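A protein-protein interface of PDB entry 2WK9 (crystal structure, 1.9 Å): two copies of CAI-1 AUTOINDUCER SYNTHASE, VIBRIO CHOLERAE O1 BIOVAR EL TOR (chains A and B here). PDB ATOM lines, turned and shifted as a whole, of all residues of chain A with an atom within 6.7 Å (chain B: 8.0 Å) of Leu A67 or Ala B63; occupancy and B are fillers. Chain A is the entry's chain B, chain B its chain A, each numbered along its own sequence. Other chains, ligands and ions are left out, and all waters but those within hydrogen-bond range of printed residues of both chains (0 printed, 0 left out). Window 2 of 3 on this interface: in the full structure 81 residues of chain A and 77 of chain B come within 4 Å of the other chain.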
ATOM      1  N   LYS A  59     -21.061  13.698  16.542  1.00  0.00           N
ATOM      2  CA  LYS A  59     -19.728  13.250  16.172  1.00  0.00           C
ATOM      3  C   LYS A  59     -19.783  12.338  14.945  1.00  0.00           C
ATOM      4  O   LYS A  59     -19.008  12.502  14.011  1.00  0.00           O
ATOM      5  CB  LYS A  59     -19.049  12.550  17.350  1.00  0.00           C
ATOM      6  CG  LYS A  59     -18.829  13.450  18.557  1.00  0.00           C
ATOM      7  CD  LYS A  59     -17.746  12.889  19.466  1.00  0.00           C
ATOM      8  CE  LYS A  59     -17.889  11.384  19.609  1.00  0.00           C
ATOM      9  NZ  LYS A  59     -17.012  10.833  20.679  1.00  0.00           N
ATOM     10  N   LEU A  62     -20.505  14.426  11.838  1.00  0.00           N
ATOM     11  CA  LEU A  62     -19.331  15.212  11.449  1.00  0.00           C
ATOM     12  C   LEU A  62     -18.296  14.371  10.708  1.00  0.00           C
ATOM     13  O   LEU A  62     -17.845  14.740   9.621  1.00  0.00           O
ATOM     14  CB  LEU A  62     -18.679  15.864  12.669  1.00  0.00           C
ATOM     15  CG  LEU A  62     -18.915  17.360  12.859  1.00  0.00           C
ATOM     16  CD1 LEU A  62     -18.201  17.842  14.111  1.00  0.00           C
ATOM     17  CD2 LEU A  62     -18.435  18.128  11.640  1.00  0.00           C
ATOM     18  N   ALA A  63     -17.914  13.250  11.312  1.00  0.00           N
ATOM     19  CA  ALA A  63     -16.927  12.354  10.709  1.00  0.00           C
ATOM     20  C   ALA A  63     -17.393  11.887   9.338  1.00  0.00           C
ATOM     21  O   ALA A  63     -16.641  11.931   8.369  1.00  0.00           O
ATOM     22  CB  ALA A  63     -16.654  11.165  11.621  1.00  0.00           C
ATOM     23  N   LYS A  64     -18.642  11.442   9.259  1.00  0.00           N
ATOM     24  CA  LYS A  64     -19.211  10.996   7.994  1.00  0.00           C
ATOM     25  C   LYS A  64     -18.972  12.043   6.915  1.00  0.00           C
ATOM     26  O   LYS A  64     -18.435  11.739   5.845  1.00  0.00           O
ATOM     27  CB  LYS A  64     -20.715  10.746   8.140  1.00  0.00           C
ATOM     28  CG  LYS A  64     -21.244   9.584   7.319  1.00  0.00           C
ATOM     29  CD  LYS A  64     -22.731   9.742   7.009  1.00  0.00           C
ATOM     30  CE  LYS A  64     -23.505  10.340   8.182  1.00  0.00           C
ATOM     31  NZ  LYS A  64     -23.625   9.404   9.337  1.00  0.00           N
ATOM     32  N   SER A  65     -19.368  13.280   7.205  1.00  0.00           N
ATOM     33  CA  SER A  65     -19.246  14.374   6.243  1.00  0.00           C
ATOM     34  C   SER A  65     -17.799  14.715   5.898  1.00  0.00           C
ATOM     35  O   SER A  65     -17.499  15.057   4.757  1.00  0.00           O
ATOM     36  CB  SER A  65     -19.973  15.628   6.740  1.00  0.00           C
ATOM     37  OG  SER A  65     -21.355  15.562   6.430  1.00  0.00           O
ATOM     38  N   LEU A  66     -16.907  14.628   6.877  1.00  0.00           N
ATOM     39  CA  LEU A  66     -15.508  14.961   6.628  1.00  0.00           C
ATOM     40  C   LEU A  66     -14.801  13.845   5.855  1.00  0.00           C
ATOM     41  O   LEU A  66     -13.910  14.107   5.047  1.00  0.00           O
ATOM     42  CB  LEU A  66     -14.778  15.313   7.927  1.00  0.00           C
ATOM     43  CG  LEU A  66     -14.167  14.220   8.798  1.00  0.00           C
ATOM     44  CD1 LEU A  66     -12.792  13.869   8.270  1.00  0.00           C
ATOM     45  CD2 LEU A  66     -14.063  14.722  10.220  1.00  0.00           C
ATOM     46  N   LEU A  67     -15.199  12.600   6.104  1.00  0.00           N
ATOM     47  CA  LEU A  67     -14.811  11.515   5.214  1.00  0.00           C
ATOM     48  C   LEU A  67     -15.532  11.793   3.908  1.00  0.00           C
ATOM     49  O   LEU A  67     -16.538  12.491   3.909  1.00  0.00           O
ATOM     50  CB  LEU A  67     -15.222  10.155   5.777  1.00  0.00           C
ATOM     51  CG  LEU A  67     -14.292   9.494   6.799  1.00  0.00           C
ATOM     52  CD1 LEU A  67     -12.916  10.145   6.776  1.00  0.00           C
ATOM     53  CD2 LEU A  67     -14.868   9.529   8.193  1.00  0.00           C
ATOM     54  N   GLU A  68     -15.019  11.274   2.799  1.00  0.00           N
ATOM     55  CA  GLU A  68     -15.545  11.626   1.479  1.00  0.00           C
ATOM     56  C   GLU A  68     -15.238  13.087   1.147  1.00  0.00           C
ATOM     57  O   GLU A  68     -15.601  13.584   0.076  1.00  0.00           O
ATOM     58  CB  GLU A  68     -17.057  11.388   1.397  1.00  0.00           C
ATOM     59  CG  GLU A  68     -17.902  12.632   1.659  1.00  0.00           C
ATOM     60  CD  GLU A  68     -19.378  12.320   1.809  1.00  0.00           C
ATOM     61  OE1 GLU A  68     -20.072  13.063   2.540  1.00  0.00           O
ATOM     62  OE2 GLU A  68     -19.845  11.332   1.200  1.00  0.00           O
ATOM     63  N   TYR A 271     -18.102  20.561   5.037  1.00  0.00           N
ATOM     64  CA  TYR A 271     -18.504  19.496   5.951  1.00  0.00           C
ATOM     65  C   TYR A 271     -18.881  20.040   7.328  1.00  0.00           C
ATOM     66  O   TYR A 271     -19.611  19.396   8.085  1.00  0.00           O
ATOM     67  CB  TYR A 271     -17.411  18.429   6.074  1.00  0.00           C
ATOM     68  CG  TYR A 271     -16.161  18.878   6.790  1.00  0.00           C
ATOM     69  CD1 TYR A 271     -16.085  18.860   8.177  1.00  0.00           C
ATOM     70  CD2 TYR A 271     -15.050  19.297   6.080  1.00  0.00           C
ATOM     71  CE1 TYR A 271     -14.940  19.259   8.832  1.00  0.00           C
ATOM     72  CE2 TYR A 271     -13.898  19.695   6.723  1.00  0.00           C
ATOM     73  CZ  TYR A 271     -13.847  19.676   8.097  1.00  0.00           C
ATOM     74  OH  TYR A 271     -12.696  20.077   8.733  1.00  0.00           O
ATOM     75  N   ASN B  54      -8.405  16.903   0.128  1.00  0.00           N
ATOM     76  CA  ASN B  54      -9.067  15.604   0.171  1.00  0.00           C
ATOM     77  C   ASN B  54      -8.154  14.442   0.530  1.00  0.00           C
ATOM     78  O   ASN B  54      -8.530  13.280   0.371  1.00  0.00           O
ATOM     79  CB  ASN B  54      -9.757  15.310  -1.157  1.00  0.00           C
ATOM     80  CG  ASN B  54     -11.259  15.430  -1.063  1.00  0.00           C
ATOM     81  OD1 ASN B  54     -11.975  14.428  -1.132  1.00  0.00           O
ATOM     82  ND2 ASN B  54     -11.748  16.654  -0.882  1.00  0.00           N
ATOM     83  N   HIS B  55      -6.960  14.753   1.017  1.00  0.00           N
ATOM     84  CA  HIS B  55      -5.999  13.718   1.368  1.00  0.00           C
ATOM     85  C   HIS B  55      -6.626  12.737   2.355  1.00  0.00           C
ATOM     86  O   HIS B  55      -7.095  13.136   3.418  1.00  0.00           O
ATOM     87  CB  HIS B  55      -4.735  14.340   1.956  1.00  0.00           C
ATOM     88  CG  HIS B  55      -3.555  13.424   1.944  1.00  0.00           C
ATOM     89  ND1 HIS B  55      -3.458  12.327   2.771  1.00  0.00           N
ATOM     90  CD2 HIS B  55      -2.417  13.443   1.208  1.00  0.00           C
ATOM     91  CE1 HIS B  55      -2.312  11.709   2.545  1.00  0.00           C
ATOM     92  NE2 HIS B  55      -1.662  12.366   1.602  1.00  0.00           N
ATOM     93  N   PRO B  56      -6.635  11.445   2.000  1.00  0.00           N
ATOM     94  CA  PRO B  56      -7.285  10.413   2.817  1.00  0.00           C
ATOM     95  C   PRO B  56      -6.691  10.321   4.221  1.00  0.00           C
ATOM     96  O   PRO B  56      -7.426  10.178   5.201  1.00  0.00           O
ATOM     97  CB  PRO B  56      -6.999   9.120   2.044  1.00  0.00           C
ATOM     98  CG  PRO B  56      -6.651   9.557   0.661  1.00  0.00           C
ATOM     99  CD  PRO B  56      -5.991  10.885   0.801  1.00  0.00           C
ATOM    100  N   LEU B  57      -5.371  10.410   4.315  1.00  0.00           N
ATOM    101  CA  LEU B  57      -4.705  10.281   5.603  1.00  0.00           C
ATOM    102  C   LEU B  57      -5.125  11.400   6.560  1.00  0.00           C
ATOM    103  O   LEU B  57      -5.337  11.165   7.745  1.00  0.00           O
ATOM    104  CB  LEU B  57      -3.187  10.258   5.428  1.00  0.00           C
ATOM    105  CG  LEU B  57      -2.398   9.824   6.662  1.00  0.00           C
ATOM    106  CD1 LEU B  57      -2.812   8.423   7.103  1.00  0.00           C
ATOM    107  CD2 LEU B  57      -0.905   9.892   6.388  1.00  0.00           C
ATOM    108  N   ILE B  58      -5.242  12.620   6.043  1.00  0.00           N
ATOM    109  CA  ILE B  58      -5.667  13.744   6.872  1.00  0.00           C
ATOM    110  C   ILE B  58      -7.117  13.567   7.314  1.00  0.00           C
ATOM    111  O   ILE B  58      -7.449  13.755   8.483  1.00  0.00           O
ATOM    112  CB  ILE B  58      -5.505  15.091   6.138  1.00  0.00           C
ATOM    113  CG1 ILE B  58      -4.024  15.368   5.865  1.00  0.00           C
ATOM    114  CG2 ILE B  58      -6.118  16.223   6.955  1.00  0.00           C
ATOM    115  CD1 ILE B  58      -3.768  16.520   4.912  1.00  0.00           C
ATOM    116  N   LYS B  59      -7.983  13.196   6.378  1.00  0.00           N
ATOM    117  CA  LYS B  59      -9.389  13.016   6.706  1.00  0.00           C
ATOM    118  C   LYS B  59      -9.568  11.908   7.743  1.00  0.00           C
ATOM    119  O   LYS B  59     -10.359  12.037   8.668  1.00  0.00           O
ATOM    120  CB  LYS B  59     -10.205  12.735   5.443  1.00  0.00           C
ATOM    121  CG  LYS B  59     -10.014  13.799   4.368  1.00  0.00           C
ATOM    122  CD  LYS B  59     -11.165  13.823   3.379  1.00  0.00           C
ATOM    123  CE  LYS B  59     -11.291  12.505   2.641  1.00  0.00           C
ATOM    124  NZ  LYS B  59     -12.347  12.576   1.596  1.00  0.00           N
ATOM    125  N   ALA B  60      -8.805  10.830   7.594  1.00  0.00           N
ATOM    126  CA  ALA B  60      -8.909   9.696   8.506  1.00  0.00           C
ATOM    127  C   ALA B  60      -8.465  10.082   9.903  1.00  0.00           C
ATOM    128  O   ALA B  60      -9.067   9.670  10.889  1.00  0.00           O
ATOM    129  CB  ALA B  60      -8.092   8.521   7.992  1.00  0.00           C
ATOM    130  N   ARG B  61      -7.407  10.886   9.990  1.00  0.00           N
ATOM    131  CA  ARG B  61      -6.885  11.301  11.286  1.00  0.00           C
ATOM    132  C   ARG B  61      -7.819  12.280  11.991  1.00  0.00           C
ATOM    133  O   ARG B  61      -8.006  12.204  13.208  1.00  0.00           O
ATOM    134  CB  ARG B  61      -5.492  11.906  11.132  1.00  0.00           C
ATOM    135  CG  ARG B  61      -4.501  10.970  10.462  1.00  0.00           C
ATOM    136  CD  ARG B  61      -4.171   9.768  11.336  1.00  0.00           C
ATOM    137  NE  ARG B  61      -3.255   8.847  10.665  1.00  0.00           N
ATOM    138  CZ  ARG B  61      -1.941   9.033  10.571  1.00  0.00           C
ATOM    139  NH1 ARG B  61      -1.379  10.115  11.096  1.00  0.00           N
ATOM    140  NH2 ARG B  61      -1.186   8.139   9.943  1.00  0.00           N
ATOM    141  N   LEU B  62      -8.388  13.211  11.231  1.00  0.00           N
ATOM    142  CA  LEU B  62      -9.360  14.145  11.788  1.00  0.00           C
ATOM    143  C   LEU B  62     -10.563  13.372  12.302  1.00  0.00           C
ATOM    144  O   LEU B  62     -11.025  13.590  13.424  1.00  0.00           O
ATOM    145  CB  LEU B  62      -9.833  15.136  10.727  1.00  0.00           C
ATOM    146  CG  LEU B  62      -9.171  16.503  10.617  1.00  0.00           C
ATOM    147  CD1 LEU B  62      -9.812  17.275   9.482  1.00  0.00           C
ATOM    148  CD2 LEU B  62      -9.299  17.266  11.931  1.00  0.00           C
ATOM    149  N   ALA B  63     -11.077  12.480  11.458  1.00  0.00           N
ATOM    150  CA  ALA B  63     -12.234  11.667  11.827  1.00  0.00           C
ATOM    151  C   ALA B  63     -11.960  10.899  13.113  1.00  0.00           C
ATOM    152  O   ALA B  63     -12.781  10.894  14.035  1.00  0.00           O
ATOM    153  CB  ALA B  63     -12.593  10.716  10.700  1.00  0.00           C
ATOM    154  N   LYS B  64     -10.793  10.262  13.177  1.00  0.00           N
ATOM    155  CA  LYS B  64     -10.417   9.468  14.343  1.00  0.00           C
ATOM    156  C   LYS B  64     -10.428  10.265  15.651  1.00  0.00           C
ATOM    157  O   LYS B  64     -11.146   9.915  16.586  1.00  0.00           O
ATOM    158  CB  LYS B  64      -9.052   8.807  14.138  1.00  0.00           C
ATOM    159  CG  LYS B  64      -8.720   7.774  15.200  1.00  0.00           C
ATOM    160  CD  LYS B  64      -7.272   7.338  15.138  1.00  0.00           C
ATOM    161  CE  LYS B  64      -6.383   8.268  15.947  1.00  0.00           C
ATOM    162  NZ  LYS B  64      -6.785   8.290  17.386  1.00  0.00           N
ATOM    163  N   SER B  65      -9.630  11.330  15.726  1.00  0.00           N
ATOM    164  CA  SER B  65      -9.569  12.136  16.949  1.00  0.00           C
ATOM    165  C   SER B  65     -10.930  12.743  17.275  1.00  0.00           C
ATOM    166  O   SER B  65     -11.275  12.920  18.436  1.00  0.00           O
ATOM    167  CB  SER B  65      -8.504  13.239  16.843  1.00  0.00           C
ATOM    168  OG  SER B  65      -8.793  14.124  15.775  1.00  0.00           O
ATOM    169  N   LEU B  66     -11.692  13.049  16.230  1.00  0.00           N
ATOM    170  CA  LEU B  66     -13.047  13.576  16.353  1.00  0.00           C
ATOM    171  C   LEU B  66     -13.964  12.661  17.172  1.00  0.00           C
ATOM    172  O   LEU B  66     -15.105  13.019  17.458  1.00  0.00           O
ATOM    173  CB  LEU B  66     -13.625  13.795  14.955  1.00  0.00           C
ATOM    174  CG  LEU B  66     -14.826  14.708  14.728  1.00  0.00           C
ATOM    175  CD1 LEU B  66     -14.651  15.462  13.420  1.00  0.00           C
ATOM    176  CD2 LEU B  66     -16.116  13.914  14.725  1.00  0.00           C
ATOM    177  N   LEU B  67     -13.470  11.482  17.545  1.00  0.00           N
ATOM    178  CA  LEU B  67     -14.203  10.607  18.461  1.00  0.00           C
ATOM    179  C   LEU B  67     -13.486  10.503  19.817  1.00  0.00           C
ATOM    180  O   LEU B  67     -12.384   9.964  19.888  1.00  0.00           O
ATOM    181  CB  LEU B  67     -14.393   9.218  17.851  1.00  0.00           C
ATOM    182  CG  LEU B  67     -14.420   9.053  16.325  1.00  0.00           C
ATOM    183  CD1 LEU B  67     -14.676   7.601  15.966  1.00  0.00           C
ATOM    184  CD2 LEU B  67     -15.461   9.933  15.662  1.00  0.00           C
ATOM    185  N   GLU B  68     -14.114  11.051  20.866  1.00  0.00           N
ATOM    186  CA  GLU B  68     -13.670  10.954  22.271  1.00  0.00           C
ATOM    187  C   GLU B  68     -13.461  12.317  22.952  1.00  0.00           C
ATOM    188  O   GLU B  68     -12.408  12.588  23.536  1.00  0.00           O
ATOM    189  CB  GLU B  68     -12.426  10.074  22.434  1.00  0.00           C
ATOM    190  CG  GLU B  68     -12.714   8.578  22.388  1.00  0.00           C
ATOM    191  CD  GLU B  68     -11.592   7.752  22.980  1.00  0.00           C
ATOM    192  OE1 GLU B  68     -10.853   8.279  23.841  1.00  0.00           O
ATOM    193  OE2 GLU B  68     -11.453   6.576  22.588  1.00  0.00           O
ATOM    194  N   GLU B  69     -14.489  13.157  22.900  1.00  0.00           N
ATOM    195  CA  GLU B  69     -14.355  14.549  23.311  1.00  0.00           C
ATOM    196  C   GLU B  69     -14.658  14.774  24.784  1.00  0.00           C
ATOM    197  O   GLU B  69     -15.551  15.553  25.122  1.00  0.00           O
ATOM    198  CB  GLU B  69     -15.259  15.448  22.460  1.00  0.00           C
ATOM    199  CG  GLU B  69     -15.149  15.198  20.967  1.00  0.00           C
ATOM    200  CD  GLU B  69     -13.711  15.032  20.520  1.00  0.00           C
ATOM    201  OE1 GLU B  69     -13.447  14.131  19.696  1.00  0.00           O
ATOM    202  OE2 GLU B  69     -12.846  15.792  21.004  1.00  0.00           O
ATOM    203  N   TYR B 271      -9.469  18.175  18.675  1.00  0.00           N
ATOM    204  CA  TYR B 271      -9.402  17.294  17.511  1.00  0.00           C
ATOM    205  C   TYR B 271      -8.922  18.028  16.257  1.00  0.00           C
ATOM    206  O   TYR B 271      -8.417  17.410  15.317  1.00  0.00           O
ATOM    207  CB  TYR B 271     -10.742  16.595  17.264  1.00  0.00           C
ATOM    208  CG  TYR B 271     -11.797  17.444  16.594  1.00  0.00           C
ATOM    209  CD1 TYR B 271     -11.845  17.569  15.211  1.00  0.00           C
ATOM    210  CD2 TYR B 271     -12.764  18.099  17.342  1.00  0.00           C
ATOM    211  CE1 TYR B 271     -12.820  18.338  14.596  1.00  0.00           C
ATOM    212  CE2 TYR B 271     -13.735  18.868  16.737  1.00  0.00           C
ATOM    213  CZ  TYR B 271     -13.762  18.979  15.369  1.00  0.00           C
ATOM    214  OH  TYR B 271     -14.739  19.740  14.778  1.00  0.00           O
ATOM    215  N   GLY B 275      -5.561  16.928  13.626  1.00  0.00           N
ATOM    216  CA  GLY B 275      -5.574  16.869  12.177  1.00  0.00           C
ATOM    217  C   GLY B 275      -4.416  17.641  11.569  1.00  0.00           C
ATOM    218  O   GLY B 275      -3.851  17.244  10.549  1.00  0.00           O
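Of chain B, only Lys B59 and Ala B63 come within 4 Å of Leu A67. Ala B63 touches just these residues of chain A: Leu A66 (3.9 Å) and Leu A67 (3.6 Å). Leu A66 touches just these residues of chain B: Lys B59, Ala B63 and Leu B66. Of the printed residues of chain B, Ala A63 touches Leu B66 (3.9 Å). Of the printed residues of chain B, Lys A59 touches Leu B66 (3.3 Å), Leu B67 (3.6 Å), Glu B68 (2.9 Å) and Glu B69 (3.8 Å). Printed residues of chain B within 4 Å of Leu A62: Leu B66. Of the printed residues of chain B, Glu A68 touches Asn B54 and Lys B59. Of the printed residues of chain A, Glu B69 touches Lys A59. His B55 touches none of the printed residues of chain A. Lys B64 touches none of the printed residues of chain A. The nearest residue of chain B that does not touch Leu A67 is Ala B60 (4.2 Å).
Lys A59 touches Leu B67, and with the chains exchanged Leu A67 touches Lys B59. Lys A59 touches Glu B68, and with the chains exchanged Glu A68 touches Lys B59. Ala A63 touches Leu B66, and with the chains exchanged Leu A66 touches Ala B63. Leu A67 touches Ala B63, but with the chains exchanged Ala A63 does not touch Leu B67 (4.4 Å). 9 positions are printed for both chains.
Leu B67 touches Lys A59 (CA to NZ, 3.6 Å). Glu B69 touches Lys A59 (CG to CD, 3.8 Å). Leu A62 touches Leu B66 (CB to CD2, 3.8 Å). Ala A63 touches Leu B66 (N to CD2, 3.9 Å). O of Lys B59 touches CD1 of Leu A66, at 3.1 Å. Ala B63 touches Leu A66 (N to CD1, 3.9 Å). CD1 of Leu B66 touches CD2 of Leu A66, at 3.3 Å. Leu A67 touches Lys B59 (CD1 to O, 3.7 Å). Leu A67 touches Ala B63 (CD2 to CB, 3.6 Å). Glu A68 touches Asn B54.
The side-chain amino group (NZ) of Lys B59 sits close to the backbone NH (N) of Glu A68 (3.2 Å). NZ of Lys A59 lies close to N of Glu B68.
Along chain B the printed residues that touch a printed residue of chain A span positions 54 to 69. Hydrophobic or aromatic side chains of chain A within 4 Å of the printed part of chain B: Leu A62, Leu A66 and Leu A67.
The side-chain amide oxygen (OD1) of Asn B54 is in hydrogen-bond range of the side-chain amino group (NZ) of Lys B59, 3.3 Å away. OE1 of Glu B69 sits at hydrogen-bond distance from N of Leu B67, 3.4 Å away.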
